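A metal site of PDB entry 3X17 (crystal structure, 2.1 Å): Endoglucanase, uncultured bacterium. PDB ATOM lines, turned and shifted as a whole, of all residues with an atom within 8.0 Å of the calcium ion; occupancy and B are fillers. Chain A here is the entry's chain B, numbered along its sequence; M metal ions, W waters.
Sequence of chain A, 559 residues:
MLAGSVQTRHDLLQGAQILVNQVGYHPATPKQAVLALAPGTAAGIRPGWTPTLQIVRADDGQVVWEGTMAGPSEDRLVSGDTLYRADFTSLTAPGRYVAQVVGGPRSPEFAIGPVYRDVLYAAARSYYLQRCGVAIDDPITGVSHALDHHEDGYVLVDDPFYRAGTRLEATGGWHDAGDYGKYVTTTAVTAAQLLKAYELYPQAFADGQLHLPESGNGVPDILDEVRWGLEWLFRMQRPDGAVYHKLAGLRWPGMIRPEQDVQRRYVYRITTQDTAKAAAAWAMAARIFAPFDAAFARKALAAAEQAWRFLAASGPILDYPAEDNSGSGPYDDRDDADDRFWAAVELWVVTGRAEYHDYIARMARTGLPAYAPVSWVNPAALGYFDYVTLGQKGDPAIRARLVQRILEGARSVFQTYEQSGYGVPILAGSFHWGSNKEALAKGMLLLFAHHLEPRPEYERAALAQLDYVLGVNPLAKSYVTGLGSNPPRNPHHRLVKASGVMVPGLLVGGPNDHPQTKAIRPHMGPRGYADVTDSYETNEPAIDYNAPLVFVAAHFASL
Within 4 Å of the calcium ion: Asp 333, Asp 335, Asp 338, Asp 339 and Val 377. The nearest printed residue that does not touch the calcium ion is Lys 277 (4.2 Å).
O of Asp 333 sits at hydrogen-bond distance from OH of Tyr 320. N of Val 377 lies close to OG of Ser 375. The side-chain carboxylate of Asp 333 lies close to the side-chain amide oxygen of Gln 273, at 3.5 Å. OD2 of Asp 333 sits close to NZ of Lys 277, 2.7 Å away. The backbone NH of Ala 337 is in hydrogen-bond range of the side-chain carboxylate of Asp 335. The side-chain carboxylate (OD1) of Asp 339 lies within salt-bridge range of the side-chain amino group (NZ) of Lys 277, at 2.6 Å.
The calcium ion is bound by the side-chain carboxylate (OD2) of Asp 339, the backbone carbonyl oxygen (O) of Asp 335, the backbone carbonyl oxygen (O) of Val 377, the side-chain carboxylate (OD1) of Asp 338, the side-chain carboxylate (OD2) of Asp 333, water W1 and the side-chain carboxylate (OD1) of Asp 333. The calcium ion has seven donor atoms within binding distance.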
ATOM      1  N   THR A 185     -32.791  13.482  22.866  1.00  0.00           N
ATOM      2  CA  THR A 185     -32.674  14.456  21.801  1.00  0.00           C
ATOM      3  C   THR A 185     -33.671  15.591  22.047  1.00  0.00           C
ATOM      4  O   THR A 185     -33.334  16.773  21.905  1.00  0.00           O
ATOM      5  CB  THR A 185     -32.909  13.780  20.402  1.00  0.00           C
ATOM      6  OG1 THR A 185     -32.016  12.658  20.265  1.00  0.00           O
ATOM      7  CG2 THR A 185     -32.668  14.769  19.258  1.00  0.00           C
ATOM      8  N   GLN A 273     -24.705  13.607  18.285  1.00  0.00           N
ATOM      9  CA  GLN A 273     -25.659  14.727  18.466  1.00  0.00           C
ATOM     10  C   GLN A 273     -26.244  14.785  19.878  1.00  0.00           C
ATOM     11  O   GLN A 273     -26.374  15.860  20.460  1.00  0.00           O
ATOM     12  CB  GLN A 273     -26.773  14.762  17.392  1.00  0.00           C
ATOM     13  CG  GLN A 273     -27.672  13.540  17.321  1.00  0.00           C
ATOM     14  CD  GLN A 273     -28.993  13.712  18.071  1.00  0.00           C
ATOM     15  OE1 GLN A 273     -29.205  14.709  18.775  1.00  0.00           O
ATOM     16  NE2 GLN A 273     -29.875  12.717  17.959  1.00  0.00           N
ATOM     17  N   ASP A 274     -26.614  13.636  20.435  1.00  0.00           N
ATOM     18  CA  ASP A 274     -27.118  13.583  21.796  1.00  0.00           C
ATOM     19  C   ASP A 274     -26.016  13.994  22.761  1.00  0.00           C
ATOM     20  O   ASP A 274     -26.293  14.683  23.753  1.00  0.00           O
ATOM     21  CB  ASP A 274     -27.667  12.192  22.152  1.00  0.00           C
ATOM     22  CG  ASP A 274     -28.995  11.879  21.466  1.00  0.00           C
ATOM     23  OD1 ASP A 274     -29.937  12.689  21.595  1.00  0.00           O
ATOM     24  OD2 ASP A 274     -29.105  10.789  20.823  1.00  0.00           O
ATOM     25  N   LYS A 277     -25.719  17.844  22.380  1.00  0.00           N
ATOM     26  CA  LYS A 277     -26.903  18.468  22.999  1.00  0.00           C
ATOM     27  C   LYS A 277     -26.846  18.430  24.517  1.00  0.00           C
ATOM     28  O   LYS A 277     -27.090  19.428  25.182  1.00  0.00           O
ATOM     29  CB  LYS A 277     -28.203  17.820  22.540  1.00  0.00           C
ATOM     30  CG  LYS A 277     -28.688  18.229  21.150  1.00  0.00           C
ATOM     31  CD  LYS A 277     -29.848  17.327  20.748  1.00  0.00           C
ATOM     32  CE  LYS A 277     -30.588  17.828  19.511  1.00  0.00           C
ATOM     33  NZ  LYS A 277     -29.924  17.301  18.276  1.00  0.00           N
ATOM     34  N   LEU A 318     -24.024   8.605  14.169  1.00  0.00           N
ATOM     35  CA  LEU A 318     -25.396   8.950  13.992  1.00  0.00           C
ATOM     36  C   LEU A 318     -26.150   7.777  13.388  1.00  0.00           C
ATOM     37  O   LEU A 318     -26.769   7.904  12.341  1.00  0.00           O
ATOM     38  CB  LEU A 318     -25.498  10.206  13.108  1.00  0.00           C
ATOM     39  CG  LEU A 318     -24.805  11.437  13.733  1.00  0.00           C
ATOM     40  CD1 LEU A 318     -24.625  12.582  12.766  1.00  0.00           C
ATOM     41  CD2 LEU A 318     -25.565  11.920  14.957  1.00  0.00           C
ATOM     42  N   TYR A 320     -29.123   5.041  13.404  1.00  0.00           N
ATOM     43  CA  TYR A 320     -30.481   4.892  13.877  1.00  0.00           C
ATOM     44  C   TYR A 320     -31.130   3.650  13.247  1.00  0.00           C
ATOM     45  O   TYR A 320     -32.004   3.762  12.398  1.00  0.00           O
ATOM     46  CB  TYR A 320     -31.317   6.153  13.576  1.00  0.00           C
ATOM     47  CG  TYR A 320     -30.726   7.443  14.152  1.00  0.00           C
ATOM     48  CD1 TYR A 320     -30.883   7.766  15.496  1.00  0.00           C
ATOM     49  CD2 TYR A 320     -30.007   8.323  13.358  1.00  0.00           C
ATOM     50  CE1 TYR A 320     -30.349   8.937  16.022  1.00  0.00           C
ATOM     51  CE2 TYR A 320     -29.436   9.468  13.875  1.00  0.00           C
ATOM     52  CZ  TYR A 320     -29.648   9.802  15.194  1.00  0.00           C
ATOM     53  OH  TYR A 320     -29.097  10.962  15.698  1.00  0.00           O
ATOM     54  N   ASP A 332     -34.164  10.821  14.580  1.00  0.00           N
ATOM     55  CA  ASP A 332     -32.967  10.466  13.841  1.00  0.00           C
ATOM     56  C   ASP A 332     -32.329  11.742  13.269  1.00  0.00           C
ATOM     57  O   ASP A 332     -32.475  12.070  12.060  1.00  0.00           O
ATOM     58  CB  ASP A 332     -33.300   9.442  12.748  1.00  0.00           C
ATOM     59  CG  ASP A 332     -34.455   9.860  11.883  1.00  0.00           C
ATOM     60  OD1 ASP A 332     -35.350  10.617  12.360  1.00  0.00           O
ATOM     61  OD2 ASP A 332     -34.455   9.473  10.699  1.00  0.00           O
ATOM     62  N   ASP A 333     -31.725  12.534  14.161  1.00  0.00           N
ATOM     63  CA  ASP A 333     -31.072  13.787  13.781  1.00  0.00           C
ATOM     64  C   ASP A 333     -29.754  13.438  13.090  1.00  0.00           C
ATOM     65  O   ASP A 333     -28.867  12.846  13.694  1.00  0.00           O
ATOM     66  CB  ASP A 333     -30.814  14.630  15.034  1.00  0.00           C
ATOM     67  CG  ASP A 333     -29.896  15.831  14.784  1.00  0.00           C
ATOM     68  OD1 ASP A 333     -29.562  16.154  13.619  1.00  0.00           O
ATOM     69  OD2 ASP A 333     -29.464  16.437  15.783  1.00  0.00           O
ATOM     70  N   ARG A 334     -29.695  13.643  11.783  1.00  0.00           N
ATOM     71  CA  ARG A 334     -28.632  13.038  10.960  1.00  0.00           C
ATOM     72  C   ARG A 334     -27.425  13.965  10.691  1.00  0.00           C
ATOM     73  O   ARG A 334     -26.578  13.641   9.860  1.00  0.00           O
ATOM     74  CB  ARG A 334     -29.226  12.399   9.687  1.00  0.00           C
ATOM     75  CG  ARG A 334     -30.360  11.423  10.062  1.00  0.00           C
ATOM     76  CD  ARG A 334     -30.790  10.426   9.008  1.00  0.00           C
ATOM     77  NE  ARG A 334     -30.191   9.118   9.263  1.00  0.00           N
ATOM     78  CZ  ARG A 334     -30.859   8.010   9.591  1.00  0.00           C
ATOM     79  NH1 ARG A 334     -32.179   8.013   9.700  1.00  0.00           N
ATOM     80  NH2 ARG A 334     -30.185   6.897   9.819  1.00  0.00           N
ATOM     81  N   ASP A 335     -27.282  14.999  11.508  1.00  0.00           N
ATOM     82  CA  ASP A 335     -26.108  15.879  11.443  1.00  0.00           C
ATOM     83  C   ASP A 335     -25.797  16.483  12.814  1.00  0.00           C
ATOM     84  O   ASP A 335     -26.671  17.119  13.421  1.00  0.00           O
ATOM     85  CB  ASP A 335     -26.350  16.984  10.400  1.00  0.00           C
ATOM     86  CG  ASP A 335     -25.156  17.926  10.212  1.00  0.00           C
ATOM     87  OD1 ASP A 335     -24.118  17.752  10.868  1.00  0.00           O
ATOM     88  OD2 ASP A 335     -25.282  18.880   9.410  1.00  0.00           O
ATOM     89  N   ASP A 336     -24.569  16.327  13.282  1.00  0.00           N
ATOM     90  CA  ASP A 336     -24.206  16.772  14.619  1.00  0.00           C
ATOM     91  C   ASP A 336     -23.460  18.111  14.691  1.00  0.00           C
ATOM     92  O   ASP A 336     -23.016  18.533  15.763  1.00  0.00           O
ATOM     93  CB  ASP A 336     -23.427  15.673  15.366  1.00  0.00           C
ATOM     94  CG  ASP A 336     -21.993  15.482  14.862  1.00  0.00           C
ATOM     95  OD1 ASP A 336     -21.530  16.313  14.048  1.00  0.00           O
ATOM     96  OD2 ASP A 336     -21.296  14.554  15.339  1.00  0.00           O
ATOM     97  N   ALA A 337     -23.259  18.748  13.539  1.00  0.00           N
ATOM     98  CA  ALA A 337     -22.419  19.969  13.503  1.00  0.00           C
ATOM     99  C   ALA A 337     -23.111  21.156  14.193  1.00  0.00           C
ATOM    100  O   ALA A 337     -22.469  21.938  14.898  1.00  0.00           O
ATOM    101  CB  ALA A 337     -22.014  20.351  12.017  1.00  0.00           C
ATOM    102  N   ASP A 338     -24.426  21.276  13.991  1.00  0.00           N
ATOM    103  CA  ASP A 338     -25.164  22.312  14.654  1.00  0.00           C
ATOM    104  C   ASP A 338     -25.242  22.091  16.152  1.00  0.00           C
ATOM    105  O   ASP A 338     -25.188  23.056  16.933  1.00  0.00           O
ATOM    106  CB  ASP A 338     -26.546  22.567  14.017  1.00  0.00           C
ATOM    107  CG  ASP A 338     -27.360  21.300  13.844  1.00  0.00           C
ATOM    108  OD1 ASP A 338     -27.113  20.312  14.578  1.00  0.00           O
ATOM    109  OD2 ASP A 338     -28.268  21.299  12.978  1.00  0.00           O
ATOM    110  N   ASP A 339     -25.366  20.836  16.552  1.00  0.00           N
ATOM    111  CA  ASP A 339     -25.268  20.443  17.968  1.00  0.00           C
ATOM    112  C   ASP A 339     -23.881  20.684  18.587  1.00  0.00           C
ATOM    113  O   ASP A 339     -23.771  21.212  19.692  1.00  0.00           O
ATOM    114  CB  ASP A 339     -25.711  18.974  18.138  1.00  0.00           C
ATOM    115  CG  ASP A 339     -26.984  18.676  17.374  1.00  0.00           C
ATOM    116  OD1 ASP A 339     -28.057  18.999  17.894  1.00  0.00           O
ATOM    117  OD2 ASP A 339     -26.926  18.128  16.251  1.00  0.00           O
ATOM    118  N   ARG A 340     -22.810  20.324  17.864  1.00  0.00           N
ATOM    119  CA  ARG A 340     -21.445  20.628  18.362  1.00  0.00           C
ATOM    120  C   ARG A 340     -21.183  22.125  18.478  1.00  0.00           C
ATOM    121  O   ARG A 340     -20.592  22.585  19.463  1.00  0.00           O
ATOM    122  CB  ARG A 340     -20.346  19.990  17.508  1.00  0.00           C
ATOM    123  CG  ARG A 340     -20.372  18.481  17.462  1.00  0.00           C
ATOM    124  CD  ARG A 340     -19.287  17.954  16.498  1.00  0.00           C
ATOM    125  NE  ARG A 340     -19.364  16.509  16.316  1.00  0.00           N
ATOM    126  CZ  ARG A 340     -18.406  15.635  16.647  1.00  0.00           C
ATOM    127  NH1 ARG A 340     -17.287  16.050  17.202  1.00  0.00           N
ATOM    128  NH2 ARG A 340     -18.591  14.346  16.427  1.00  0.00           N
ATOM    129  N   SER A 375     -35.044  23.598  17.281  1.00  0.00           N
ATOM    130  CA  SER A 375     -35.699  22.286  17.165  1.00  0.00           C
ATOM    131  C   SER A 375     -34.734  21.185  17.618  1.00  0.00           C
ATOM    132  O   SER A 375     -33.549  21.436  17.771  1.00  0.00           O
ATOM    133  CB  SER A 375     -36.116  22.037  15.695  1.00  0.00           C
ATOM    134  OG  SER A 375     -34.984  21.680  14.927  1.00  0.00           O
ATOM    135  N   TRP A 376     -35.236  19.969  17.846  1.00  0.00           N
ATOM    136  CA  TRP A 376     -34.380  18.816  18.163  1.00  0.00           C
ATOM    137  C   TRP A 376     -33.435  18.393  17.032  1.00  0.00           C
ATOM    138  O   TRP A 376     -32.441  17.708  17.266  1.00  0.00           O
ATOM    139  CB  TRP A 376     -35.221  17.618  18.630  1.00  0.00           C
ATOM    140  CG  TRP A 376     -36.180  17.049  17.604  1.00  0.00           C
ATOM    141  CD1 TRP A 376     -37.534  17.274  17.536  1.00  0.00           C
ATOM    142  CD2 TRP A 376     -35.889  16.094  16.575  1.00  0.00           C
ATOM    143  NE1 TRP A 376     -38.077  16.619  16.452  1.00  0.00           N
ATOM    144  CE2 TRP A 376     -37.095  15.877  15.848  1.00  0.00           C
ATOM    145  CE3 TRP A 376     -34.725  15.479  16.130  1.00  0.00           C
ATOM    146  CZ2 TRP A 376     -37.181  15.000  14.764  1.00  0.00           C
ATOM    147  CZ3 TRP A 376     -34.798  14.600  15.024  1.00  0.00           C
ATOM    148  CH2 TRP A 376     -36.024  14.364  14.364  1.00  0.00           C
ATOM    149  N   VAL A 377     -33.708  18.853  15.816  1.00  0.00           N
ATOM    150  CA  VAL A 377     -32.762  18.683  14.714  1.00  0.00           C
ATOM    151  C   VAL A 377     -31.622  19.701  14.810  1.00  0.00           C
ATOM    152  O   VAL A 377     -30.429  19.336  14.858  1.00  0.00           O
ATOM    153  CB  VAL A 377     -33.456  18.789  13.352  1.00  0.00           C
ATOM    154  CG1 VAL A 377     -32.452  18.753  12.209  1.00  0.00           C
ATOM    155  CG2 VAL A 377     -34.491  17.654  13.177  1.00  0.00           C
ATOM    156  N   ASN A 378     -32.006  20.983  14.867  1.00  0.00           N
ATOM    157  CA  ASN A 378     -31.061  22.093  14.862  1.00  0.00           C
ATOM    158  C   ASN A 378     -31.346  23.053  16.022  1.00  0.00           C
ATOM    159  O   ASN A 378     -32.337  23.761  16.018  1.00  0.00           O
ATOM    160  CB  ASN A 378     -31.156  22.852  13.540  1.00  0.00           C
ATOM    161  CG  ASN A 378     -30.182  23.988  13.449  1.00  0.00           C
ATOM    162  OD1 ASN A 378     -29.547  24.368  14.430  1.00  0.00           O
ATOM    163  ND2 ASN A 378     -30.093  24.588  12.273  1.00  0.00           N
ATOM    164  N   PRO A 379     -30.560  22.968  17.078  1.00  0.00           N
ATOM    165  CA  PRO A 379     -30.744  23.818  18.248  1.00  0.00           C
ATOM    166  C   PRO A 379     -29.817  25.058  18.209  1.00  0.00           C
ATOM    167  O   PRO A 379     -29.708  25.792  19.203  1.00  0.00           O
ATOM    168  CB  PRO A 379     -30.317  22.896  19.388  1.00  0.00           C
ATOM    169  CG  PRO A 379     -29.223  22.134  18.820  1.00  0.00           C
ATOM    170  CD  PRO A 379     -29.636  21.851  17.365  1.00  0.00           C
ATOM    171  N   ALA A 380     -29.094  25.250  17.113  1.00  0.00           N
ATOM    172  CA  ALA A 380     -27.975  26.170  17.131  1.00  0.00           C
ATOM    173  C   ALA A 380     -28.358  27.654  17.336  1.00  0.00           C
ATOM    174  O   ALA A 380     -27.492  28.452  17.667  1.00  0.00           O
ATOM    175  CB  ALA A 380     -27.092  25.996  15.862  1.00  0.00           C
HETATM  176 CA    CA M   1     -28.325  18.223  14.489  1.00  0.00          CA
HETATM  177  O   HOH W   1     -28.769  19.133  12.209  1.00  0.00           O
